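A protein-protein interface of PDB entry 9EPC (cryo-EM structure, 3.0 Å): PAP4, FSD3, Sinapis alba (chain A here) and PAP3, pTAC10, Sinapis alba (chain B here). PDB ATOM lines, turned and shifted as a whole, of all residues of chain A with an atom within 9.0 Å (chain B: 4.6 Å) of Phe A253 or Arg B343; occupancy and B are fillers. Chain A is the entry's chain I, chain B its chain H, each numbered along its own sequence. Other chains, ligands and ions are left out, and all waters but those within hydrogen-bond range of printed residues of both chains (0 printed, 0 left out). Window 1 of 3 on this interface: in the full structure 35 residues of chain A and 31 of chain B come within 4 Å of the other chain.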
ATOM      1  N   GLU A 103      -1.994 -13.387 -15.239  1.00  0.00           N
ATOM      2  CA  GLU A 103      -2.041 -12.856 -13.881  1.00  0.00           C
ATOM      3  C   GLU A 103      -2.894 -13.734 -12.979  1.00  0.00           C
ATOM      4  O   GLU A 103      -2.560 -13.948 -11.808  1.00  0.00           O
ATOM      5  CB  GLU A 103      -2.569 -11.421 -13.894  1.00  0.00           C
ATOM      6  CG  GLU A 103      -1.609 -10.399 -14.492  1.00  0.00           C
ATOM      7  CD  GLU A 103      -1.508 -10.492 -16.003  1.00  0.00           C
ATOM      8  OE1 GLU A 103      -2.299 -11.242 -16.612  1.00  0.00           O
ATOM      9  OE2 GLU A 103      -0.634  -9.813 -16.582  1.00  0.00           O
ATOM     10  N   LEU A 182       4.431  -1.621  -7.877  1.00  0.00           N
ATOM     11  CA  LEU A 182       3.481  -0.617  -7.432  1.00  0.00           C
ATOM     12  C   LEU A 182       2.455  -1.284  -6.529  1.00  0.00           C
ATOM     13  O   LEU A 182       1.852  -2.292  -6.911  1.00  0.00           O
ATOM     14  CB  LEU A 182       2.795   0.042  -8.628  1.00  0.00           C
ATOM     15  CG  LEU A 182       2.039   1.340  -8.364  1.00  0.00           C
ATOM     16  CD1 LEU A 182       2.986   2.388  -7.818  1.00  0.00           C
ATOM     17  CD2 LEU A 182       1.377   1.828  -9.637  1.00  0.00           C
ATOM     18  N   LYS A 183       2.271  -0.734  -5.335  1.00  0.00           N
ATOM     19  CA  LYS A 183       1.321  -1.277  -4.374  1.00  0.00           C
ATOM     20  C   LYS A 183      -0.070  -0.730  -4.662  1.00  0.00           C
ATOM     21  O   LYS A 183      -0.251   0.486  -4.773  1.00  0.00           O
ATOM     22  CB  LYS A 183       1.745  -0.928  -2.948  1.00  0.00           C
ATOM     23  CG  LYS A 183       3.058  -1.553  -2.518  1.00  0.00           C
ATOM     24  CD  LYS A 183       2.942  -3.062  -2.431  1.00  0.00           C
ATOM     25  CE  LYS A 183       4.208  -3.681  -1.872  1.00  0.00           C
ATOM     26  NZ  LYS A 183       4.082  -5.157  -1.723  1.00  0.00           N
ATOM     27  N   ARG A 184      -1.048  -1.629  -4.787  1.00  0.00           N
ATOM     28  CA  ARG A 184      -2.413  -1.194  -5.073  1.00  0.00           C
ATOM     29  C   ARG A 184      -2.993  -0.404  -3.908  1.00  0.00           C
ATOM     30  O   ARG A 184      -3.517   0.701  -4.090  1.00  0.00           O
ATOM     31  CB  ARG A 184      -3.297  -2.400  -5.385  1.00  0.00           C
ATOM     32  CG  ARG A 184      -2.964  -3.112  -6.678  1.00  0.00           C
ATOM     33  CD  ARG A 184      -3.903  -4.285  -6.891  1.00  0.00           C
ATOM     34  NE  ARG A 184      -3.579  -5.032  -8.099  1.00  0.00           N
ATOM     35  CZ  ARG A 184      -4.128  -4.809  -9.285  1.00  0.00           C
ATOM     36  NH1 ARG A 184      -5.038  -3.867  -9.458  1.00  0.00           N
ATOM     37  NH2 ARG A 184      -3.755  -5.553 -10.322  1.00  0.00           N
ATOM     38  N   GLU A 185      -2.909  -0.958  -2.698  1.00  0.00           N
ATOM     39  CA  GLU A 185      -3.498  -0.289  -1.543  1.00  0.00           C
ATOM     40  C   GLU A 185      -2.663   0.907  -1.108  1.00  0.00           C
ATOM     41  O   GLU A 185      -3.207   1.971  -0.795  1.00  0.00           O
ATOM     42  CB  GLU A 185      -3.663  -1.279  -0.389  1.00  0.00           C
ATOM     43  CG  GLU A 185      -4.807  -2.272  -0.565  1.00  0.00           C
ATOM     44  CD  GLU A 185      -4.535  -3.313  -1.634  1.00  0.00           C
ATOM     45  OE1 GLU A 185      -3.364  -3.460  -2.045  1.00  0.00           O
ATOM     46  OE2 GLU A 185      -5.495  -3.987  -2.065  1.00  0.00           O
ATOM     47  N   ARG A 187      -0.495   2.576  -2.953  1.00  0.00           N
ATOM     48  CA  ARG A 187      -0.404   3.548  -4.044  1.00  0.00           C
ATOM     49  C   ARG A 187       0.984   4.178  -4.128  1.00  0.00           C
ATOM     50  O   ARG A 187       1.125   5.388  -4.317  1.00  0.00           O
ATOM     51  CB  ARG A 187      -1.480   4.625  -3.902  1.00  0.00           C
ATOM     52  CG  ARG A 187      -2.897   4.096  -4.008  1.00  0.00           C
ATOM     53  CD  ARG A 187      -3.882   5.027  -3.327  1.00  0.00           C
ATOM     54  NE  ARG A 187      -3.622   6.426  -3.641  1.00  0.00           N
ATOM     55  CZ  ARG A 187      -4.030   7.033  -4.746  1.00  0.00           C
ATOM     56  NH1 ARG A 187      -4.709   6.386  -5.679  1.00  0.00           N
ATOM     57  NH2 ARG A 187      -3.747   8.320  -4.920  1.00  0.00           N
ATOM     58  N   ASP A 204      -1.116  -9.252  -5.635  1.00  0.00           N
ATOM     59  CA  ASP A 204      -1.822  -8.289  -6.476  1.00  0.00           C
ATOM     60  C   ASP A 204      -0.970  -7.080  -6.840  1.00  0.00           C
ATOM     61  O   ASP A 204      -1.454  -6.197  -7.554  1.00  0.00           O
ATOM     62  CB  ASP A 204      -3.131  -7.802  -5.839  1.00  0.00           C
ATOM     63  CG  ASP A 204      -4.168  -8.899  -5.731  1.00  0.00           C
ATOM     64  OD1 ASP A 204      -4.286  -9.700  -6.681  1.00  0.00           O
ATOM     65  OD2 ASP A 204      -4.863  -8.964  -4.696  1.00  0.00           O
ATOM     66  N   ASP A 205       0.275  -7.008  -6.381  1.00  0.00           N
ATOM     67  CA  ASP A 205       1.146  -5.908  -6.764  1.00  0.00           C
ATOM     68  C   ASP A 205       1.486  -5.994  -8.245  1.00  0.00           C
ATOM     69  O   ASP A 205       1.561  -7.078  -8.828  1.00  0.00           O
ATOM     70  CB  ASP A 205       2.420  -5.920  -5.925  1.00  0.00           C
ATOM     71  CG  ASP A 205       2.137  -5.811  -4.442  1.00  0.00           C
ATOM     72  OD1 ASP A 205       1.078  -5.257  -4.081  1.00  0.00           O
ATOM     73  OD2 ASP A 205       2.971  -6.275  -3.638  1.00  0.00           O
ATOM     74  N   ILE A 206       1.691  -4.831  -8.856  1.00  0.00           N
ATOM     75  CA  ILE A 206       1.908  -4.722 -10.296  1.00  0.00           C
ATOM     76  C   ILE A 206       3.399  -4.498 -10.528  1.00  0.00           C
ATOM     77  O   ILE A 206       3.911  -3.419 -10.187  1.00  0.00           O
ATOM     78  CB  ILE A 206       1.076  -3.586 -10.901  1.00  0.00           C
ATOM     79  CG1 ILE A 206      -0.398  -3.769 -10.541  1.00  0.00           C
ATOM     80  CG2 ILE A 206       1.262  -3.541 -12.405  1.00  0.00           C
ATOM     81  CD1 ILE A 206      -1.215  -2.508 -10.665  1.00  0.00           C
ATOM     82  N   ARG A 246       4.668   0.059 -18.471  1.00  0.00           N
ATOM     83  CA  ARG A 246       4.159  -0.737 -17.361  1.00  0.00           C
ATOM     84  C   ARG A 246       3.479   0.150 -16.328  1.00  0.00           C
ATOM     85  O   ARG A 246       2.492  -0.253 -15.704  1.00  0.00           O
ATOM     86  CB  ARG A 246       5.292  -1.536 -16.723  1.00  0.00           C
ATOM     87  CG  ARG A 246       5.787  -2.697 -17.565  1.00  0.00           C
ATOM     88  CD  ARG A 246       7.301  -2.688 -17.670  1.00  0.00           C
ATOM     89  NE  ARG A 246       7.862  -4.032 -17.677  1.00  0.00           N
ATOM     90  CZ  ARG A 246       7.949  -4.806 -18.750  1.00  0.00           C
ATOM     91  NH1 ARG A 246       7.521  -4.396 -19.932  1.00  0.00           N
ATOM     92  NH2 ARG A 246       8.475  -6.020 -18.632  1.00  0.00           N
ATOM     93  N   MET A 247       4.004   1.361 -16.128  1.00  0.00           N
ATOM     94  CA  MET A 247       3.337   2.326 -15.262  1.00  0.00           C
ATOM     95  C   MET A 247       1.987   2.741 -15.830  1.00  0.00           C
ATOM     96  O   MET A 247       1.013   2.888 -15.084  1.00  0.00           O
ATOM     97  CB  MET A 247       4.226   3.551 -15.062  1.00  0.00           C
ATOM     98  CG  MET A 247       5.113   3.490 -13.840  1.00  0.00           C
ATOM     99  SD  MET A 247       4.164   3.592 -12.316  1.00  0.00           S
ATOM    100  CE  MET A 247       5.455   4.043 -11.168  1.00  0.00           C
ATOM    101  N   ALA A 248       1.913   2.941 -17.148  1.00  0.00           N
ATOM    102  CA  ALA A 248       0.665   3.381 -17.763  1.00  0.00           C
ATOM    103  C   ALA A 248      -0.444   2.360 -17.544  1.00  0.00           C
ATOM    104  O   ALA A 248      -1.576   2.720 -17.205  1.00  0.00           O
ATOM    105  CB  ALA A 248       0.878   3.638 -19.253  1.00  0.00           C
ATOM    106  N   ARG A 249      -0.136   1.077 -17.738  1.00  0.00           N
ATOM    107  CA  ARG A 249      -1.114   0.040 -17.425  1.00  0.00           C
ATOM    108  C   ARG A 249      -1.403  -0.007 -15.931  1.00  0.00           C
ATOM    109  O   ARG A 249      -2.557  -0.171 -15.522  1.00  0.00           O
ATOM    110  CB  ARG A 249      -0.621  -1.317 -17.923  1.00  0.00           C
ATOM    111  CG  ARG A 249      -1.410  -2.493 -17.382  1.00  0.00           C
ATOM    112  CD  ARG A 249      -1.688  -3.516 -18.463  1.00  0.00           C
ATOM    113  NE  ARG A 249      -2.719  -3.061 -19.388  1.00  0.00           N
ATOM    114  CZ  ARG A 249      -4.013  -3.305 -19.241  1.00  0.00           C
ATOM    115  NH1 ARG A 249      -4.473  -4.001 -18.215  1.00  0.00           N
ATOM    116  NH2 ARG A 249      -4.868  -2.839 -20.147  1.00  0.00           N
ATOM    117  N   ALA A 250      -0.368   0.137 -15.101  1.00  0.00           N
ATOM    118  CA  ALA A 250      -0.577   0.158 -13.659  1.00  0.00           C
ATOM    119  C   ALA A 250      -1.422   1.355 -13.244  1.00  0.00           C
ATOM    120  O   ALA A 250      -2.280   1.244 -12.362  1.00  0.00           O
ATOM    121  CB  ALA A 250       0.766   0.170 -12.932  1.00  0.00           C
ATOM    122  N   GLU A 251      -1.191   2.510 -13.873  1.00  0.00           N
ATOM    123  CA  GLU A 251      -1.983   3.698 -13.579  1.00  0.00           C
ATOM    124  C   GLU A 251      -3.466   3.471 -13.834  1.00  0.00           C
ATOM    125  O   GLU A 251      -4.303   4.120 -13.198  1.00  0.00           O
ATOM    126  CB  GLU A 251      -1.464   4.878 -14.406  1.00  0.00           C
ATOM    127  CG  GLU A 251      -2.235   6.178 -14.239  1.00  0.00           C
ATOM    128  CD  GLU A 251      -3.323   6.350 -15.282  1.00  0.00           C
ATOM    129  OE1 GLU A 251      -3.451   5.473 -16.161  1.00  0.00           O
ATOM    130  OE2 GLU A 251      -4.051   7.364 -15.223  1.00  0.00           O
ATOM    131  N   ALA A 252      -3.811   2.551 -14.735  1.00  0.00           N
ATOM    132  CA  ALA A 252      -5.208   2.214 -14.964  1.00  0.00           C
ATOM    133  C   ALA A 252      -5.847   1.512 -13.776  1.00  0.00           C
ATOM    134  O   ALA A 252      -7.074   1.373 -13.751  1.00  0.00           O
ATOM    135  CB  ALA A 252      -5.338   1.337 -16.210  1.00  0.00           C
ATOM    136  N   PHE A 253      -5.057   1.073 -12.797  1.00  0.00           N
ATOM    137  CA  PHE A 253      -5.578   0.337 -11.657  1.00  0.00           C
ATOM    138  C   PHE A 253      -5.221   0.935 -10.305  1.00  0.00           C
ATOM    139  O   PHE A 253      -5.784   0.498  -9.294  1.00  0.00           O
ATOM    140  CB  PHE A 253      -5.083  -1.117 -11.688  1.00  0.00           C
ATOM    141  CG  PHE A 253      -5.469  -1.862 -12.930  1.00  0.00           C
ATOM    142  CD1 PHE A 253      -6.725  -1.706 -13.485  1.00  0.00           C
ATOM    143  CD2 PHE A 253      -4.572  -2.714 -13.547  1.00  0.00           C
ATOM    144  CE1 PHE A 253      -7.082  -2.390 -14.629  1.00  0.00           C
ATOM    145  CE2 PHE A 253      -4.921  -3.400 -14.692  1.00  0.00           C
ATOM    146  CZ  PHE A 253      -6.177  -3.237 -15.234  1.00  0.00           C
ATOM    147  N   VAL A 254      -4.310   1.905 -10.241  1.00  0.00           N
ATOM    148  CA  VAL A 254      -3.871   2.421  -8.949  1.00  0.00           C
ATOM    149  C   VAL A 254      -4.165   3.912  -8.829  1.00  0.00           C
ATOM    150  O   VAL A 254      -4.424   4.412  -7.727  1.00  0.00           O
ATOM    151  CB  VAL A 254      -2.374   2.135  -8.729  1.00  0.00           C
ATOM    152  CG1 VAL A 254      -1.950   2.545  -7.331  1.00  0.00           C
ATOM    153  CG2 VAL A 254      -2.084   0.663  -8.954  1.00  0.00           C
ATOM    154  N   ASN A 255      -4.158   4.625  -9.956  1.00  0.00           N
ATOM    155  CA  ASN A 255      -4.441   6.062  -9.991  1.00  0.00           C
ATOM    156  C   ASN A 255      -3.510   6.823  -9.041  1.00  0.00           C
ATOM    157  O   ASN A 255      -3.920   7.375  -8.018  1.00  0.00           O
ATOM    158  CB  ASN A 255      -5.913   6.346  -9.666  1.00  0.00           C
ATOM    159  CG  ASN A 255      -6.319   7.773  -9.992  1.00  0.00           C
ATOM    160  OD1 ASN A 255      -5.480   8.668 -10.084  1.00  0.00           O
ATOM    161  ND2 ASN A 255      -7.614   7.991 -10.168  1.00  0.00           N
ATOM    162  N   LEU A 256      -2.230   6.825  -9.409  1.00  0.00           N
ATOM    163  CA  LEU A 256      -1.195   7.481  -8.617  1.00  0.00           C
ATOM    164  C   LEU A 256      -1.392   8.990  -8.517  1.00  0.00           C
ATOM    165  O   LEU A 256      -0.622   9.673  -7.837  1.00  0.00           O
ATOM    166  CB  LEU A 256       0.182   7.183  -9.209  1.00  0.00           C
ATOM    167  CG  LEU A 256       0.583   5.711  -9.224  1.00  0.00           C
ATOM    168  CD1 LEU A 256       1.942   5.539  -9.874  1.00  0.00           C
ATOM    169  CD2 LEU A 256       0.586   5.161  -7.812  1.00  0.00           C
ATOM    170  N   VAL B 303     -18.265  -1.708 -15.313  1.00  0.00           N
ATOM    171  CA  VAL B 303     -17.078  -0.895 -15.074  1.00  0.00           C
ATOM    172  C   VAL B 303     -17.122  -0.420 -13.627  1.00  0.00           C
ATOM    173  O   VAL B 303     -18.031   0.331 -13.256  1.00  0.00           O
ATOM    174  CB  VAL B 303     -16.997   0.294 -16.040  1.00  0.00           C
ATOM    175  CG1 VAL B 303     -15.741   1.094 -15.772  1.00  0.00           C
ATOM    176  CG2 VAL B 303     -17.029  -0.193 -17.473  1.00  0.00           C
ATOM    177  N   VAL B 325     -14.528  -0.627 -25.071  1.00  0.00           N
ATOM    178  CA  VAL B 325     -14.262  -1.119 -23.728  1.00  0.00           C
ATOM    179  C   VAL B 325     -13.406  -2.375 -23.810  1.00  0.00           C
ATOM    180  O   VAL B 325     -13.423  -3.101 -24.809  1.00  0.00           O
ATOM    181  CB  VAL B 325     -15.579  -1.389 -22.970  1.00  0.00           C
ATOM    182  CG1 VAL B 325     -16.222  -2.673 -23.457  1.00  0.00           C
ATOM    183  CG2 VAL B 325     -15.342  -1.421 -21.477  1.00  0.00           C
ATOM    184  N   GLU B 326     -12.643  -2.618 -22.751  1.00  0.00           N
ATOM    185  CA  GLU B 326     -11.764  -3.774 -22.645  1.00  0.00           C
ATOM    186  C   GLU B 326     -12.247  -4.669 -21.517  1.00  0.00           C
ATOM    187  O   GLU B 326     -12.515  -4.189 -20.411  1.00  0.00           O
ATOM    188  CB  GLU B 326     -10.321  -3.341 -22.384  1.00  0.00           C
ATOM    189  CG  GLU B 326      -9.382  -4.485 -22.048  1.00  0.00           C
ATOM    190  CD  GLU B 326      -8.079  -4.007 -21.437  1.00  0.00           C
ATOM    191  OE1 GLU B 326      -7.962  -2.798 -21.151  1.00  0.00           O
ATOM    192  OE2 GLU B 326      -7.171  -4.842 -21.241  1.00  0.00           O
ATOM    193  N   THR B 328     -11.753  -6.949 -18.563  1.00  0.00           N
ATOM    194  CA  THR B 328     -10.688  -7.165 -17.595  1.00  0.00           C
ATOM    195  C   THR B 328     -10.746  -8.554 -16.977  1.00  0.00           C
ATOM    196  O   THR B 328      -9.715  -9.226 -16.866  1.00  0.00           O
ATOM    197  CB  THR B 328     -10.756  -6.105 -16.493  1.00  0.00           C
ATOM    198  OG1 THR B 328     -10.614  -4.803 -17.073  1.00  0.00           O
ATOM    199  CG2 THR B 328      -9.649  -6.321 -15.479  1.00  0.00           C
ATOM    200  N   LEU B 342     -15.271  -4.907 -16.745  1.00  0.00           N
ATOM    201  CA  LEU B 342     -14.793  -4.196 -17.922  1.00  0.00           C
ATOM    202  C   LEU B 342     -13.871  -3.048 -17.514  1.00  0.00           C
ATOM    203  O   LEU B 342     -13.564  -2.853 -16.335  1.00  0.00           O
ATOM    204  CB  LEU B 342     -15.974  -3.697 -18.755  1.00  0.00           C
ATOM    205  CG  LEU B 342     -16.506  -4.589 -19.877  1.00  0.00           C
ATOM    206  CD1 LEU B 342     -16.815  -5.988 -19.384  1.00  0.00           C
ATOM    207  CD2 LEU B 342     -17.745  -3.961 -20.476  1.00  0.00           C
ATOM    208  N   ARG B 343     -13.428  -2.287 -18.513  1.00  0.00           N
ATOM    209  CA  ARG B 343     -12.540  -1.148 -18.292  1.00  0.00           C
ATOM    210  C   ARG B 343     -12.624  -0.242 -19.507  1.00  0.00           C
ATOM    211  O   ARG B 343     -12.328  -0.681 -20.622  1.00  0.00           O
ATOM    212  CB  ARG B 343     -11.104  -1.608 -18.068  1.00  0.00           C
ATOM    213  CG  ARG B 343     -10.158  -0.493 -17.668  1.00  0.00           C
ATOM    214  CD  ARG B 343      -8.711  -0.873 -17.919  1.00  0.00           C
ATOM    215  NE  ARG B 343      -8.348  -0.719 -19.321  1.00  0.00           N
ATOM    216  CZ  ARG B 343      -7.938   0.421 -19.863  1.00  0.00           C
ATOM    217  NH1 ARG B 343      -7.834   1.528 -19.148  1.00  0.00           N
ATOM    218  NH2 ARG B 343      -7.628   0.449 -21.155  1.00  0.00           N
ATOM    219  N   PHE B 344     -13.019   1.012 -19.300  1.00  0.00           N
ATOM    220  CA  PHE B 344     -13.146   1.944 -20.412  1.00  0.00           C
ATOM    221  C   PHE B 344     -11.791   2.202 -21.054  1.00  0.00           C
ATOM    222  O   PHE B 344     -10.804   2.468 -20.362  1.00  0.00           O
ATOM    223  CB  PHE B 344     -13.747   3.265 -19.940  1.00  0.00           C
ATOM    224  CG  PHE B 344     -15.229   3.222 -19.746  1.00  0.00           C
ATOM    225  CD1 PHE B 344     -16.075   3.076 -20.827  1.00  0.00           C
ATOM    226  CD2 PHE B 344     -15.778   3.347 -18.486  1.00  0.00           C
ATOM    227  CE1 PHE B 344     -17.439   3.040 -20.652  1.00  0.00           C
ATOM    228  CE2 PHE B 344     -17.141   3.315 -18.308  1.00  0.00           C
ATOM    229  CZ  PHE B 344     -17.973   3.161 -19.392  1.00  0.00           C
ATOM    230  N   VAL B 345     -11.746   2.127 -22.380  1.00  0.00           N
ATOM    231  CA  VAL B 345     -10.586   2.583 -23.131  1.00  0.00           C
ATOM    232  C   VAL B 345     -10.902   3.801 -23.989  1.00  0.00           C
ATOM    233  O   VAL B 345      -9.966   4.474 -24.444  1.00  0.00           O
ATOM    234  CB  VAL B 345      -9.991   1.456 -24.000  1.00  0.00           C
ATOM    235  CG1 VAL B 345     -10.186   0.113 -23.330  1.00  0.00           C
ATOM    236  CG2 VAL B 345     -10.598   1.463 -25.385  1.00  0.00           C
ATOM    237  N   ASN B 348     -11.007   7.593 -21.753  1.00  0.00           N
ATOM    238  CA  ASN B 348     -10.150   7.048 -20.710  1.00  0.00           C
ATOM    239  C   ASN B 348     -10.508   7.696 -19.380  1.00  0.00           C
ATOM    240  O   ASN B 348     -10.341   8.907 -19.208  1.00  0.00           O
ATOM    241  CB  ASN B 348      -8.679   7.282 -21.044  1.00  0.00           C
ATOM    242  CG  ASN B 348      -7.746   6.583 -20.081  1.00  0.00           C
ATOM    243  OD1 ASN B 348      -7.403   7.122 -19.032  1.00  0.00           O
ATOM    244  ND2 ASN B 348      -7.327   5.376 -20.436  1.00  0.00           N
ATOM    245  N   ASP B 350      -9.274   6.359 -16.423  1.00  0.00           N
ATOM    246  CA  ASP B 350      -8.358   5.807 -15.434  1.00  0.00           C
ATOM    247  C   ASP B 350      -7.694   6.876 -14.580  1.00  0.00           C
ATOM    248  O   ASP B 350      -7.153   6.553 -13.517  1.00  0.00           O
ATOM    249  CB  ASP B 350      -7.300   4.958 -16.133  1.00  0.00           C
ATOM    250  CG  ASP B 350      -7.909   3.905 -17.035  1.00  0.00           C
ATOM    251  OD1 ASP B 350      -8.149   4.205 -18.223  1.00  0.00           O
ATOM    252  OD2 ASP B 350      -8.166   2.783 -16.553  1.00  0.00           O
ATOM    253  N   LYS B 356     -11.641   2.135  -5.472  1.00  0.00           N
ATOM    254  CA  LYS B 356     -11.462   0.843  -6.112  1.00  0.00           C
ATOM    255  C   LYS B 356     -12.123  -0.245  -5.282  1.00  0.00           C
ATOM    256  O   LYS B 356     -12.050  -0.231  -4.050  1.00  0.00           O
ATOM    257  CB  LYS B 356      -9.978   0.522  -6.294  1.00  0.00           C
ATOM    258  CG  LYS B 356      -9.163   1.660  -6.879  1.00  0.00           C
ATOM    259  CD  LYS B 356      -9.606   1.992  -8.290  1.00  0.00           C
ATOM    260  CE  LYS B 356      -9.401   0.811  -9.219  1.00  0.00           C
ATOM    261  NZ  LYS B 356      -9.796   1.135 -10.615  1.00  0.00           N
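OE2 of Glu B326 lies within salt-bridge range of NH2 of Arg A249, at 3.2 Å. The side-chain carboxylate of Asp B350 lies close to the backbone carbonyl oxygen of Ala A252, 3.3 Å away.
The side-chain carboxylate (OE1) of Glu B326 lies within salt-bridge range of the guanidinium group (NE) of Arg B343, 2.8 Å away. The side-chain carboxylate (OD1) of Asp B350 lies within salt-bridge range of the guanidinium group (NH1) of Arg B343, at 2.8 Å. The side-chain amide nitrogen (ND2) of Asn B348 sits at hydrogen-bond distance from the side-chain carboxylate (OD1) of Asp B350. The guanidinium group (NH1) of Arg A187 is in hydrogen-bond range of the backbone carbonyl oxygen (O) of Asn A255 (2.7 Å).
Of the 20 printed residues of chain A, 5 touch a printed residue of chain B. Hydrophobic or aromatic side chains of chain A that line the printed part of chain B: Ala A252 and Phe A253. Of the 11 printed residues of chain B, 4 touch a printed residue of chain A. Among the printed residues, 7 pairs touch across the chains. Among the printed residues, Asp or Glu carboxylates within 4 Å of a Lys or Arg side-chain nitrogen of the other chain: Arg A249 with Glu B326.
Leu A182 touches none of the printed residues of chain B. Of the printed residues of chain B, Arg A249 touches Glu B326 (3.2 Å). Of the printed residues of chain B, Ala A252 touches Arg B343 and Asp B350. Of chain B, only Arg B343 and Lys B356 come within 4 Å of Phe A253. Of the printed residues of chain A, Glu B326 touches Arg A249 (3.2 Å). Of chain A, only Ala A252 (3.9 Å) and Phe A253 (3.97 Å) come within 4 Å of Arg B343. Of the printed residues of chain A, Asp B350 touches Glu A251 (3.6 Å), Ala A252 (3.2 Å) and Asn A255 (3.7 Å). The nearest printed residue of chain B that does not touch Phe A253 is Thr B328 (4.7 Å). The nearest printed residue of chain A that does not touch Lys B356 is Ala A252 (4.2 Å).
O of Asp B350 touches OE2 of Glu A251 (3.6 Å). Ala A252 touches Arg B343 (CB to NH1, 3.9 Å). CE1 of Phe A253 touches CD of Arg B343, at 3.97 Å. Lys B356 touches Phe A253. Asn A255 touches Asp B350.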
